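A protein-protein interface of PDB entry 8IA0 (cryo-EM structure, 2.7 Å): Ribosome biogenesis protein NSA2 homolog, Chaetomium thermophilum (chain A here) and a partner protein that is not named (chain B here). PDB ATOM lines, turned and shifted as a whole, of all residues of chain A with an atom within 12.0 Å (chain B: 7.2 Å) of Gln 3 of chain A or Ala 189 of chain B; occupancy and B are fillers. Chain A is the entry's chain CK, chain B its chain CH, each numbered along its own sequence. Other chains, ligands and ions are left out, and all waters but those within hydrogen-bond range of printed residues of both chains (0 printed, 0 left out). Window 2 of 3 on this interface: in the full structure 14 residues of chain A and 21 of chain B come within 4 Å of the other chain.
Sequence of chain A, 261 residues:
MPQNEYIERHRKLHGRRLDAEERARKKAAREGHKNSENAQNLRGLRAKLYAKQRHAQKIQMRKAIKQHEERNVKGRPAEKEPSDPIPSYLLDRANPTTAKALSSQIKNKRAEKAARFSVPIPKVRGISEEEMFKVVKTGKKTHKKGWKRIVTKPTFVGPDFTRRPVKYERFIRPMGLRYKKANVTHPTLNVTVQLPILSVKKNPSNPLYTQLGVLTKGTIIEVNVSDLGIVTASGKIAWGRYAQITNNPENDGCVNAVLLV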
ATOM      1  N   PRO A   2     -20.079   3.353  18.447  1.00  0.00           N
ATOM      2  CA  PRO A   2     -19.275   3.289  19.668  1.00  0.00           C
ATOM      3  C   PRO A   2     -18.686   4.651  20.029  1.00  0.00           C
ATOM      4  O   PRO A   2     -18.573   5.511  19.158  1.00  0.00           O
ATOM      5  CB  PRO A   2     -18.189   2.277  19.314  1.00  0.00           C
ATOM      6  CG  PRO A   2     -18.141   2.238  17.805  1.00  0.00           C
ATOM      7  CD  PRO A   2     -19.288   3.025  17.253  1.00  0.00           C
ATOM      8  N   GLN A   3     -18.314   4.844  21.297  1.00  0.00           N
ATOM      9  CA  GLN A   3     -18.096   6.189  21.810  1.00  0.00           C
ATOM     10  C   GLN A   3     -16.847   6.368  22.661  1.00  0.00           C
ATOM     11  O   GLN A   3     -16.620   7.479  23.150  1.00  0.00           O
ATOM     12  CB  GLN A   3     -19.314   6.627  22.634  1.00  0.00           C
ATOM     13  CG  GLN A   3     -19.794   5.566  23.599  1.00  0.00           C
ATOM     14  CD  GLN A   3     -21.126   5.900  24.219  1.00  0.00           C
ATOM     15  OE1 GLN A   3     -21.520   7.063  24.284  1.00  0.00           O
ATOM     16  NE2 GLN A   3     -21.835   4.879  24.682  1.00  0.00           N
ATOM     17  N   ASN A   4     -16.048   5.332  22.868  1.00  0.00           N
ATOM     18  CA  ASN A   4     -14.853   5.427  23.699  1.00  0.00           C
ATOM     19  C   ASN A   4     -13.853   4.405  23.175  1.00  0.00           C
ATOM     20  O   ASN A   4     -13.907   4.017  22.006  1.00  0.00           O
ATOM     21  CB  ASN A   4     -15.211   5.266  25.185  1.00  0.00           C
ATOM     22  CG  ASN A   4     -15.715   6.557  25.794  1.00  0.00           C
ATOM     23  OD1 ASN A   4     -14.968   7.524  25.917  1.00  0.00           O
ATOM     24  ND2 ASN A   4     -16.991   6.590  26.153  1.00  0.00           N
ATOM     25  N   GLU A   5     -12.914   3.990  24.019  1.00  0.00           N
ATOM     26  CA  GLU A   5     -11.897   3.055  23.562  1.00  0.00           C
ATOM     27  C   GLU A   5     -12.548   1.704  23.289  1.00  0.00           C
ATOM     28  O   GLU A   5     -12.424   0.778  24.095  1.00  0.00           O
ATOM     29  CB  GLU A   5     -10.794   2.911  24.612  1.00  0.00           C
ATOM     30  CG  GLU A   5     -10.017   4.186  24.882  1.00  0.00           C
ATOM     31  CD  GLU A   5      -9.027   4.516  23.790  1.00  0.00           C
ATOM     32  OE1 GLU A   5      -7.882   4.018  23.846  1.00  0.00           O
ATOM     33  OE2 GLU A   5      -9.394   5.281  22.876  1.00  0.00           O
ATOM     34  N   TYR A   6     -13.245   1.581  22.151  1.00  0.00           N
ATOM     35  CA  TYR A   6     -14.145   0.448  21.957  1.00  0.00           C
ATOM     36  C   TYR A   6     -13.428  -0.826  21.525  1.00  0.00           C
ATOM     37  O   TYR A   6     -13.877  -1.922  21.877  1.00  0.00           O
ATOM     38  CB  TYR A   6     -15.250   0.785  20.946  1.00  0.00           C
ATOM     39  CG  TYR A   6     -14.841   1.519  19.683  1.00  0.00           C
ATOM     40  CD1 TYR A   6     -14.412   0.826  18.562  1.00  0.00           C
ATOM     41  CD2 TYR A   6     -14.942   2.897  19.593  1.00  0.00           C
ATOM     42  CE1 TYR A   6     -14.062   1.490  17.403  1.00  0.00           C
ATOM     43  CE2 TYR A   6     -14.597   3.568  18.442  1.00  0.00           C
ATOM     44  CZ  TYR A   6     -14.157   2.863  17.351  1.00  0.00           C
ATOM     45  OH  TYR A   6     -13.811   3.536  16.204  1.00  0.00           O
ATOM     46  N   ILE A   7     -12.337  -0.724  20.766  1.00  0.00           N
ATOM     47  CA  ILE A   7     -11.643  -1.933  20.331  1.00  0.00           C
ATOM     48  C   ILE A   7     -11.039  -2.666  21.522  1.00  0.00           C
ATOM     49  O   ILE A   7     -11.119  -3.896  21.614  1.00  0.00           O
ATOM     50  CB  ILE A   7     -10.583  -1.598  19.265  1.00  0.00           C
ATOM     51  CG1 ILE A   7     -11.254  -1.184  17.953  1.00  0.00           C
ATOM     52  CG2 ILE A   7      -9.670  -2.785  19.023  1.00  0.00           C
ATOM     53  CD1 ILE A   7     -12.094  -2.267  17.319  1.00  0.00           C
ATOM     54  N   GLU A   8     -10.427  -1.930  22.455  1.00  0.00           N
ATOM     55  CA  GLU A   8      -9.913  -2.569  23.663  1.00  0.00           C
ATOM     56  C   GLU A   8     -11.041  -3.159  24.498  1.00  0.00           C
ATOM     57  O   GLU A   8     -10.883  -4.226  25.099  1.00  0.00           O
ATOM     58  CB  GLU A   8      -9.086  -1.583  24.489  1.00  0.00           C
ATOM     59  CG  GLU A   8      -8.199  -0.667  23.670  1.00  0.00           C
ATOM     60  CD  GLU A   8      -7.440   0.329  24.524  1.00  0.00           C
ATOM     61  OE1 GLU A   8      -6.982   1.354  23.979  1.00  0.00           O
ATOM     62  OE2 GLU A   8      -7.294   0.080  25.739  1.00  0.00           O
ATOM     63  N   ARG A   9     -12.184  -2.472  24.561  1.00  0.00           N
ATOM     64  CA  ARG A   9     -13.339  -3.039  25.249  1.00  0.00           C
ATOM     65  C   ARG A   9     -13.809  -4.315  24.564  1.00  0.00           C
ATOM     66  O   ARG A   9     -14.202  -5.279  25.232  1.00  0.00           O
ATOM     67  CB  ARG A   9     -14.469  -2.015  25.316  1.00  0.00           C
ATOM     68  CG  ARG A   9     -15.718  -2.538  25.995  1.00  0.00           C
ATOM     69  CD  ARG A   9     -15.766  -2.127  27.452  1.00  0.00           C
ATOM     70  NE  ARG A   9     -17.040  -2.476  28.070  1.00  0.00           N
ATOM     71  CZ  ARG A   9     -17.167  -3.279  29.117  1.00  0.00           C
ATOM     72  NH1 ARG A   9     -16.114  -3.835  29.693  1.00  0.00           N
ATOM     73  NH2 ARG A   9     -18.380  -3.531  29.597  1.00  0.00           N
ATOM     74  N   HIS A  10     -13.783  -4.337  23.230  1.00  0.00           N
ATOM     75  CA  HIS A  10     -14.141  -5.548  22.501  1.00  0.00           C
ATOM     76  C   HIS A  10     -13.159  -6.677  22.786  1.00  0.00           C
ATOM     77  O   HIS A  10     -13.559  -7.838  22.923  1.00  0.00           O
ATOM     78  CB  HIS A  10     -14.207  -5.255  21.004  1.00  0.00           C
ATOM     79  CG  HIS A  10     -14.656  -6.419  20.177  1.00  0.00           C
ATOM     80  ND1 HIS A  10     -15.967  -6.838  20.136  1.00  0.00           N
ATOM     81  CD2 HIS A  10     -13.970  -7.247  19.356  1.00  0.00           C
ATOM     82  CE1 HIS A  10     -16.069  -7.877  19.327  1.00  0.00           C
ATOM     83  NE2 HIS A  10     -14.871  -8.147  18.842  1.00  0.00           N
ATOM     84  N   LEU A  13     -14.006  -8.168  26.249  1.00  0.00           N
ATOM     85  CA  LEU A  13     -15.232  -8.955  26.320  1.00  0.00           C
ATOM     86  C   LEU A  13     -15.160 -10.213  25.463  1.00  0.00           C
ATOM     87  O   LEU A  13     -15.695 -11.259  25.850  1.00  0.00           O
ATOM     88  CB  LEU A  13     -16.424  -8.098  25.898  1.00  0.00           C
ATOM     89  CG  LEU A  13     -17.046  -7.220  26.983  1.00  0.00           C
ATOM     90  CD1 LEU A  13     -18.245  -6.467  26.434  1.00  0.00           C
ATOM     91  CD2 LEU A  13     -17.436  -8.053  28.191  1.00  0.00           C
ATOM     92  N   HIS B 155      -8.398  10.376  19.151  1.00  0.00           N
ATOM     93  CA  HIS B 155      -9.297  10.591  20.280  1.00  0.00           C
ATOM     94  C   HIS B 155     -10.580  11.286  19.842  1.00  0.00           C
ATOM     95  O   HIS B 155     -11.671  10.941  20.308  1.00  0.00           O
ATOM     96  CB  HIS B 155      -8.587  11.402  21.362  1.00  0.00           C
ATOM     97  CG  HIS B 155      -9.093  11.141  22.745  1.00  0.00           C
ATOM     98  ND1 HIS B 155     -10.003  11.964  23.371  1.00  0.00           N
ATOM     99  CD2 HIS B 155      -8.813  10.151  23.625  1.00  0.00           C
ATOM    100  CE1 HIS B 155     -10.265  11.491  24.576  1.00  0.00           C
ATOM    101  NE2 HIS B 155      -9.556  10.392  24.755  1.00  0.00           N
ATOM    102  N   ALA B 157     -11.990  11.150  16.914  1.00  0.00           N
ATOM    103  CA  ALA B 157     -12.801  10.257  16.097  1.00  0.00           C
ATOM    104  C   ALA B 157     -13.656   9.333  16.948  1.00  0.00           C
ATOM    105  O   ALA B 157     -14.689   8.839  16.484  1.00  0.00           O
ATOM    106  CB  ALA B 157     -11.905   9.442  15.166  1.00  0.00           C
ATOM    107  N   ARG B 158     -13.247   9.086  18.187  1.00  0.00           N
ATOM    108  CA  ARG B 158     -13.969   8.181  19.066  1.00  0.00           C
ATOM    109  C   ARG B 158     -14.879   8.898  20.054  1.00  0.00           C
ATOM    110  O   ARG B 158     -15.597   8.228  20.797  1.00  0.00           O
ATOM    111  CB  ARG B 158     -12.978   7.301  19.831  1.00  0.00           C
ATOM    112  CG  ARG B 158     -12.273   6.282  18.959  1.00  0.00           C
ATOM    113  CD  ARG B 158     -11.372   5.382  19.776  1.00  0.00           C
ATOM    114  NE  ARG B 158     -10.445   6.144  20.603  1.00  0.00           N
ATOM    115  CZ  ARG B 158      -9.217   6.477  20.235  1.00  0.00           C
ATOM    116  NH1 ARG B 158      -8.735   6.141  19.052  1.00  0.00           N
ATOM    117  NH2 ARG B 158      -8.452   7.163  21.078  1.00  0.00           N
ATOM    118  N   LEU B 159     -14.875  10.228  20.077  1.00  0.00           N
ATOM    119  CA  LEU B 159     -15.671  10.958  21.052  1.00  0.00           C
ATOM    120  C   LEU B 159     -17.162  10.737  20.804  1.00  0.00           C
ATOM    121  O   LEU B 159     -17.606  10.664  19.655  1.00  0.00           O
ATOM    122  CB  LEU B 159     -15.356  12.450  20.995  1.00  0.00           C
ATOM    123  CG  LEU B 159     -14.256  12.971  21.918  1.00  0.00           C
ATOM    124  CD1 LEU B 159     -14.034  14.455  21.686  1.00  0.00           C
ATOM    125  CD2 LEU B 159     -14.594  12.699  23.370  1.00  0.00           C
ATOM    126  N   PRO B 160     -17.957  10.623  21.865  1.00  0.00           N
ATOM    127  CA  PRO B 160     -19.404  10.491  21.692  1.00  0.00           C
ATOM    128  C   PRO B 160     -20.018  11.773  21.158  1.00  0.00           C
ATOM    129  O   PRO B 160     -19.515  12.878  21.372  1.00  0.00           O
ATOM    130  CB  PRO B 160     -19.896  10.187  23.108  1.00  0.00           C
ATOM    131  CG  PRO B 160     -18.894  10.851  23.977  1.00  0.00           C
ATOM    132  CD  PRO B 160     -17.580  10.612  23.288  1.00  0.00           C
ATOM    133  N   ASP B 161     -21.129  11.610  20.449  1.00  0.00           N
ATOM    134  CA  ASP B 161     -21.860  12.727  19.865  1.00  0.00           C
ATOM    135  C   ASP B 161     -22.924  13.183  20.855  1.00  0.00           C
ATOM    136  O   ASP B 161     -23.951  12.518  21.024  1.00  0.00           O
ATOM    137  CB  ASP B 161     -22.487  12.334  18.533  1.00  0.00           C
ATOM    138  CG  ASP B 161     -23.133  13.505  17.826  1.00  0.00           C
ATOM    139  OD1 ASP B 161     -22.485  14.566  17.719  1.00  0.00           O
ATOM    140  OD2 ASP B 161     -24.289  13.364  17.374  1.00  0.00           O
ATOM    141  N   ILE B 162     -22.678  14.318  21.502  1.00  0.00           N
ATOM    142  CA  ILE B 162     -23.599  14.897  22.471  1.00  0.00           C
ATOM    143  C   ILE B 162     -24.238  16.124  21.843  1.00  0.00           C
ATOM    144  O   ILE B 162     -23.534  17.046  21.417  1.00  0.00           O
ATOM    145  CB  ILE B 162     -22.886  15.271  23.782  1.00  0.00           C
ATOM    146  CG1 ILE B 162     -22.026  14.106  24.272  1.00  0.00           C
ATOM    147  CG2 ILE B 162     -23.898  15.690  24.830  1.00  0.00           C
ATOM    148  CD1 ILE B 162     -21.553  14.247  25.697  1.00  0.00           C
ATOM    149  N   SER B 180     -23.393   4.111  36.451  1.00  0.00           N
ATOM    150  CA  SER B 180     -23.277   3.326  35.228  1.00  0.00           C
ATOM    151  C   SER B 180     -24.335   2.232  35.169  1.00  0.00           C
ATOM    152  O   SER B 180     -24.841   1.910  34.088  1.00  0.00           O
ATOM    153  CB  SER B 180     -21.875   2.729  35.121  1.00  0.00           C
ATOM    154  OG  SER B 180     -20.887   3.743  35.184  1.00  0.00           O
ATOM    155  N   VAL B 183     -27.597   3.767  33.886  1.00  0.00           N
ATOM    156  CA  VAL B 183     -27.584   4.037  32.451  1.00  0.00           C
ATOM    157  C   VAL B 183     -27.771   2.747  31.662  1.00  0.00           C
ATOM    158  O   VAL B 183     -28.517   2.708  30.676  1.00  0.00           O
ATOM    159  CB  VAL B 183     -26.284   4.763  32.058  1.00  0.00           C
ATOM    160  CG1 VAL B 183     -26.093   4.741  30.551  1.00  0.00           C
ATOM    161  CG2 VAL B 183     -26.300   6.191  32.570  1.00  0.00           C
ATOM    162  N   ARG B 184     -27.101   1.673  32.084  1.00  0.00           N
ATOM    163  CA  ARG B 184     -27.252   0.388  31.410  1.00  0.00           C
ATOM    164  C   ARG B 184     -28.689  -0.111  31.485  1.00  0.00           C
ATOM    165  O   ARG B 184     -29.152  -0.832  30.595  1.00  0.00           O
ATOM    166  CB  ARG B 184     -26.307  -0.641  32.026  1.00  0.00           C
ATOM    167  CG  ARG B 184     -24.838  -0.386  31.772  1.00  0.00           C
ATOM    168  CD  ARG B 184     -24.019  -1.638  32.033  1.00  0.00           C
ATOM    169  NE  ARG B 184     -24.199  -2.640  30.992  1.00  0.00           N
ATOM    170  CZ  ARG B 184     -23.255  -3.007  30.136  1.00  0.00           C
ATOM    171  NH1 ARG B 184     -22.046  -2.473  30.171  1.00  0.00           N
ATOM    172  NH2 ARG B 184     -23.533  -3.930  29.220  1.00  0.00           N
ATOM    173  N   SER B 185     -29.407   0.258  32.547  1.00  0.00           N
ATOM    174  CA  SER B 185     -30.758  -0.256  32.743  1.00  0.00           C
ATOM    175  C   SER B 185     -31.749   0.378  31.775  1.00  0.00           C
ATOM    176  O   SER B 185     -32.656  -0.299  31.278  1.00  0.00           O
ATOM    177  CB  SER B 185     -31.198  -0.023  34.187  1.00  0.00           C
ATOM    178  OG  SER B 185     -30.484  -0.860  35.078  1.00  0.00           O
ATOM    179  N   VAL B 186     -31.596   1.669  31.492  1.00  0.00           N
ATOM    180  CA  VAL B 186     -32.590   2.372  30.690  1.00  0.00           C
ATOM    181  C   VAL B 186     -32.157   2.533  29.234  1.00  0.00           C
ATOM    182  O   VAL B 186     -33.011   2.653  28.349  1.00  0.00           O
ATOM    183  CB  VAL B 186     -32.907   3.736  31.320  1.00  0.00           C
ATOM    184  CG1 VAL B 186     -33.743   3.555  32.575  1.00  0.00           C
ATOM    185  CG2 VAL B 186     -31.627   4.493  31.627  1.00  0.00           C
ATOM    186  N   THR B 187     -30.857   2.542  28.961  1.00  0.00           N
ATOM    187  CA  THR B 187     -30.335   2.679  27.607  1.00  0.00           C
ATOM    188  C   THR B 187     -29.479   1.464  27.278  1.00  0.00           C
ATOM    189  O   THR B 187     -29.167   0.644  28.146  1.00  0.00           O
ATOM    190  CB  THR B 187     -29.521   3.968  27.446  1.00  0.00           C
ATOM    191  OG1 THR B 187     -28.363   3.913  28.286  1.00  0.00           O
ATOM    192  CG2 THR B 187     -30.353   5.178  27.825  1.00  0.00           C
ATOM    193  N   ARG B 188     -29.099   1.345  26.009  1.00  0.00           N
ATOM    194  CA  ARG B 188     -28.244   0.255  25.564  1.00  0.00           C
ATOM    195  C   ARG B 188     -26.800   0.685  25.349  1.00  0.00           C
ATOM    196  O   ARG B 188     -26.073   0.018  24.606  1.00  0.00           O
ATOM    197  CB  ARG B 188     -28.798  -0.372  24.282  1.00  0.00           C
ATOM    198  CG  ARG B 188     -29.285   0.619  23.249  1.00  0.00           C
ATOM    199  CD  ARG B 188     -29.930  -0.106  22.081  1.00  0.00           C
ATOM    200  NE  ARG B 188     -29.282  -1.384  21.809  1.00  0.00           N
ATOM    201  CZ  ARG B 188     -28.253  -1.544  20.986  1.00  0.00           C
ATOM    202  NH1 ARG B 188     -27.728  -0.523  20.330  1.00  0.00           N
ATOM    203  NH2 ARG B 188     -27.742  -2.760  20.817  1.00  0.00           N
ATOM    204  N   ALA B 189     -26.371   1.778  25.972  1.00  0.00           N
ATOM    205  CA  ALA B 189     -24.970   2.165  25.915  1.00  0.00           C
ATOM    206  C   ALA B 189     -24.128   1.213  26.753  1.00  0.00           C
ATOM    207  O   ALA B 189     -24.476   0.886  27.891  1.00  0.00           O
ATOM    208  CB  ALA B 189     -24.793   3.600  26.408  1.00  0.00           C
ATOM    209  N   ASP B 190     -23.010   0.769  26.185  1.00  0.00           N
ATOM    210  CA  ASP B 190     -22.124  -0.179  26.857  1.00  0.00           C
ATOM    211  C   ASP B 190     -21.203   0.601  27.783  1.00  0.00           C
ATOM    212  O   ASP B 190     -20.074   0.942  27.434  1.00  0.00           O
ATOM    213  CB  ASP B 190     -21.340  -1.001  25.843  1.00  0.00           C
ATOM    214  CG  ASP B 190     -20.362  -1.954  26.499  1.00  0.00           C
ATOM    215  OD1 ASP B 190     -20.813  -2.844  27.250  1.00  0.00           O
ATOM    216  OD2 ASP B 190     -19.145  -1.814  26.263  1.00  0.00           O
ATOM    217  N   THR B 191     -21.699   0.892  28.984  1.00  0.00           N
ATOM    218  CA  THR B 191     -20.909   1.569  29.999  1.00  0.00           C
ATOM    219  C   THR B 191     -20.400   0.547  31.000  1.00  0.00           C
ATOM    220  O   THR B 191     -21.215  -0.176  31.592  1.00  0.00           O
ATOM    221  CB  THR B 191     -21.734   2.632  30.709  1.00  0.00           C
ATOM    222  OG1 THR B 191     -22.284   3.536  29.744  1.00  0.00           O
ATOM    223  CG2 THR B 191     -20.860   3.406  31.670  1.00  0.00           C
ATOM    224  N   PRO B 192     -19.090   0.437  31.212  1.00  0.00           N
ATOM    225  CA  PRO B 192     -18.577  -0.583  32.134  1.00  0.00           C
ATOM    226  C   PRO B 192     -19.090  -0.372  33.552  1.00  0.00           C
ATOM    227  O   PRO B 192     -19.213   0.758  34.028  1.00  0.00           O
ATOM    228  CB  PRO B 192     -17.056  -0.404  32.057  1.00  0.00           C
ATOM    229  CG  PRO B 192     -16.807   0.412  30.831  1.00  0.00           C
ATOM    230  CD  PRO B 192     -18.016   1.257  30.632  1.00  0.00           C
ATOM    231  N   SER B 202     -14.615   8.559  31.107  1.00  0.00           N
ATOM    232  CA  SER B 202     -15.001   9.419  30.002  1.00  0.00           C
ATOM    233  C   SER B 202     -16.518   9.475  29.924  1.00  0.00           C
ATOM    234  O   SER B 202     -17.223   8.677  30.547  1.00  0.00           O
ATOM    235  CB  SER B 202     -14.410   8.932  28.676  1.00  0.00           C
ATOM    236  OG  SER B 202     -15.167   9.403  27.576  1.00  0.00           O
ATOM    237  N   LEU B 203     -17.014  10.438  29.154  1.00  0.00           N
ATOM    238  CA  LEU B 203     -18.452  10.626  29.025  1.00  0.00           C
ATOM    239  C   LEU B 203     -19.039   9.598  28.068  1.00  0.00           C
ATOM    240  O   LEU B 203     -18.572   9.449  26.935  1.00  0.00           O
ATOM    241  CB  LEU B 203     -18.757  12.041  28.538  1.00  0.00           C
ATOM    242  CG  LEU B 203     -18.595  13.175  29.553  1.00  0.00           C
ATOM    243  CD1 LEU B 203     -18.745  14.525  28.875  1.00  0.00           C
ATOM    244  CD2 LEU B 203     -19.591  13.031  30.693  1.00  0.00           C
ATOM    245  N   PHE B 204     -20.066   8.891  28.525  1.00  0.00           N
ATOM    246  CA  PHE B 204     -20.803   7.937  27.714  1.00  0.00           C
ATOM    247  C   PHE B 204     -22.209   8.466  27.471  1.00  0.00           C
ATOM    248  O   PHE B 204     -22.808   9.101  28.342  1.00  0.00           O
ATOM    249  CB  PHE B 204     -20.878   6.566  28.392  1.00  0.00           C
ATOM    250  CG  PHE B 204     -19.585   5.803  28.377  1.00  0.00           C
ATOM    251  CD1 PHE B 204     -18.542   6.162  29.212  1.00  0.00           C
ATOM    252  CD2 PHE B 204     -19.419   4.712  27.543  1.00  0.00           C
ATOM    253  CE1 PHE B 204     -17.356   5.458  29.205  1.00  0.00           C
ATOM    254  CE2 PHE B 204     -18.236   4.004  27.533  1.00  0.00           C
ATOM    255  CZ  PHE B 204     -17.205   4.376  28.367  1.00  0.00           C
ATOM    256  N   VAL B 205     -22.734   8.199  26.279  1.00  0.00           N
ATOM    257  CA  VAL B 205     -24.034   8.709  25.860  1.00  0.00           C
ATOM    258  C   VAL B 205     -24.945   7.534  25.546  1.00  0.00           C
ATOM    259  O   VAL B 205     -24.553   6.612  24.823  1.00  0.00           O
ATOM    260  CB  VAL B 205     -23.911   9.641  24.642  1.00  0.00           C
ATOM    261  CG1 VAL B 205     -25.277  10.161  24.235  1.00  0.00           C
ATOM    262  CG2 VAL B 205     -22.979  10.786  24.957  1.00  0.00           C
ATOM    263  N   GLY B 206     -26.159   7.564  26.104  1.00  0.00           N
ATOM    264  CA  GLY B 206     -27.181   6.603  25.764  1.00  0.00           C
ATOM    265  C   GLY B 206     -28.448   7.319  25.327  1.00  0.00           C
ATOM    266  O   GLY B 206     -28.590   8.531  25.493  1.00  0.00           O
ATOM    267  N   HIS B 207     -29.370   6.543  24.764  1.00  0.00           N
ATOM    268  CA  HIS B 207     -30.610   7.095  24.243  1.00  0.00           C
ATOM    269  C   HIS B 207     -31.786   6.236  24.675  1.00  0.00           C
ATOM    270  O   HIS B 207     -31.707   5.005  24.653  1.00  0.00           O
ATOM    271  CB  HIS B 207     -30.564   7.201  22.716  1.00  0.00           C
ATOM    272  CG  HIS B 207     -29.546   8.175  22.214  1.00  0.00           C
ATOM    273  ND1 HIS B 207     -28.304   7.786  21.765  1.00  0.00           N
ATOM    274  CD2 HIS B 207     -29.582   9.523  22.100  1.00  0.00           C
ATOM    275  CE1 HIS B 207     -27.620   8.852  21.392  1.00  0.00           C
ATOM    276  NE2 HIS B 207     -28.373   9.919  21.585  1.00  0.00           N
ATOM    277  N   VAL B 217     -29.074  10.287  27.553  1.00  0.00           N
ATOM    278  CA  VAL B 217     -28.616   9.985  28.902  1.00  0.00           C
ATOM    279  C   VAL B 217     -27.096   9.982  28.874  1.00  0.00           C
ATOM    280  O   VAL B 217     -26.489   9.266  28.071  1.00  0.00           O
ATOM    281  CB  VAL B 217     -29.156   8.641  29.412  1.00  0.00           C
ATOM    282  CG1 VAL B 217     -28.849   8.478  30.887  1.00  0.00           C
ATOM    283  CG2 VAL B 217     -30.644   8.560  29.176  1.00  0.00           C
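NE of Arg 158 of chain B is in salt-bridge range of OE2 of Glu 5 of chain A, 2.6 Å away.
The side-chain amide oxygen (OE1) of Gln 3 of chain A sits at hydrogen-bond distance from the backbone NH (N) of Val 205 of chain B (2.6 Å).
The side-chain hydroxyl of Ser 202 of chain B is in hydrogen-bond range of the side-chain amide oxygen of Asn 4 of chain A, 2.5 Å away.
The backbone carbonyl oxygen of Gln 3 of chain A sits close to the backbone carbonyl oxygen of Arg 158 of chain B (2.7 Å).
The guanidinium group (NE) of Arg 9 of chain A is in salt-bridge range of the side-chain carboxylate (OD2) of Asp 190 of chain B, 2.9 Å away.
O of Leu 203 of chain B lies within hydrogen-bond range of ND2 of Asn 4 of chain A (3.4 Å).
Pro 160 of chain B touches just one residue of chain A: Gln 3 (3.3 Å).
Of chain A, only Arg 9 comes within 4 Å of Arg 184 of chain B.
No residue of chain A comes within 4 Å of Thr 187 of chain B.
No residue of chain A comes within 4 Å of Arg 188 of chain B.
Of chain A, only Arg 9 comes within 4 Å of Asp 190 of chain B.
No residue of chain A comes within 4 Å of Thr 191 of chain B.
Of chain A, only Gln 3 and Asn 4 come within 4 Å of Phe 204 of chain B.
Val 205 of chain B touches just one residue of chain A: Gln 3 (2.6 Å).
No residue of chain A comes within 4 Å of Gly 206 of chain B.
Of the printed residues of chain A, Arg 158 of chain B touches Gln 3 (2.7 Å), Asn 4 (3.6 Å), Glu 5 (2.6 Å) and Tyr 6 (3.6 Å).
Printed residues of chain A within 4 Å of Ser 202 of chain B: Asn 4 (2.5 Å).
Of the printed residues of chain B, Asn 4 of chain A touches Arg 158 (3.6 Å), Ser 202 (2.5 Å), Leu 203 (3.4 Å) and Phe 204 (3.1 Å).
The nearest residue of chain A that does not touch Ala 189 of chain B is Arg 9 of chain A (7.7 Å).
Among the printed residues, pairs that only touch across the chains: Asn 4 of chain A with Phe 204 of chain B, Gln 3 of chain A with Pro 160 of chain B, Gln 3 of chain A with Phe 204 of chain B, Asn 4 of chain A with Arg 158 of chain B, Tyr 6 of chain A with Arg 158 of chain B, Gln 3 of chain A with Ala 189 of chain B, Arg 9 of chain A with Arg 184 of chain B and Arg 9 of chain A with Pro 192 of chain B.
NH1 of Arg 184 of chain B sits at hydrogen-bond distance from O of Thr 191 of chain B, 2.8 Å away.
The side-chain carboxylate (OD1) of Asp 190 of chain B is in salt-bridge range of the guanidinium group (NH1) of Arg 184 of chain B, 3.2 Å away.
Printed residues of chain A that touch a printed residue of chain B: Gln 3, Asn 4, Glu 5, Tyr 6 and Arg 9.
Of the 25 printed residues of chain B, 10 touch a printed residue of chain A.
Hydrophobic or aromatic side chains of chain B within 4 Å of the printed part of chain A: Pro 160, Ala 189, Phe 204 and Val 205.
Among the printed residues, 14 pairs touch across the chains.
Among the printed residues, Asp or Glu carboxylates within 4 Å of a Lys or Arg side-chain nitrogen of the other chain: Glu 5 of chain A with Arg 158 of chain B (2.6 Å) and Arg 9 of chain A with Asp 190 of chain B (2.9 Å).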
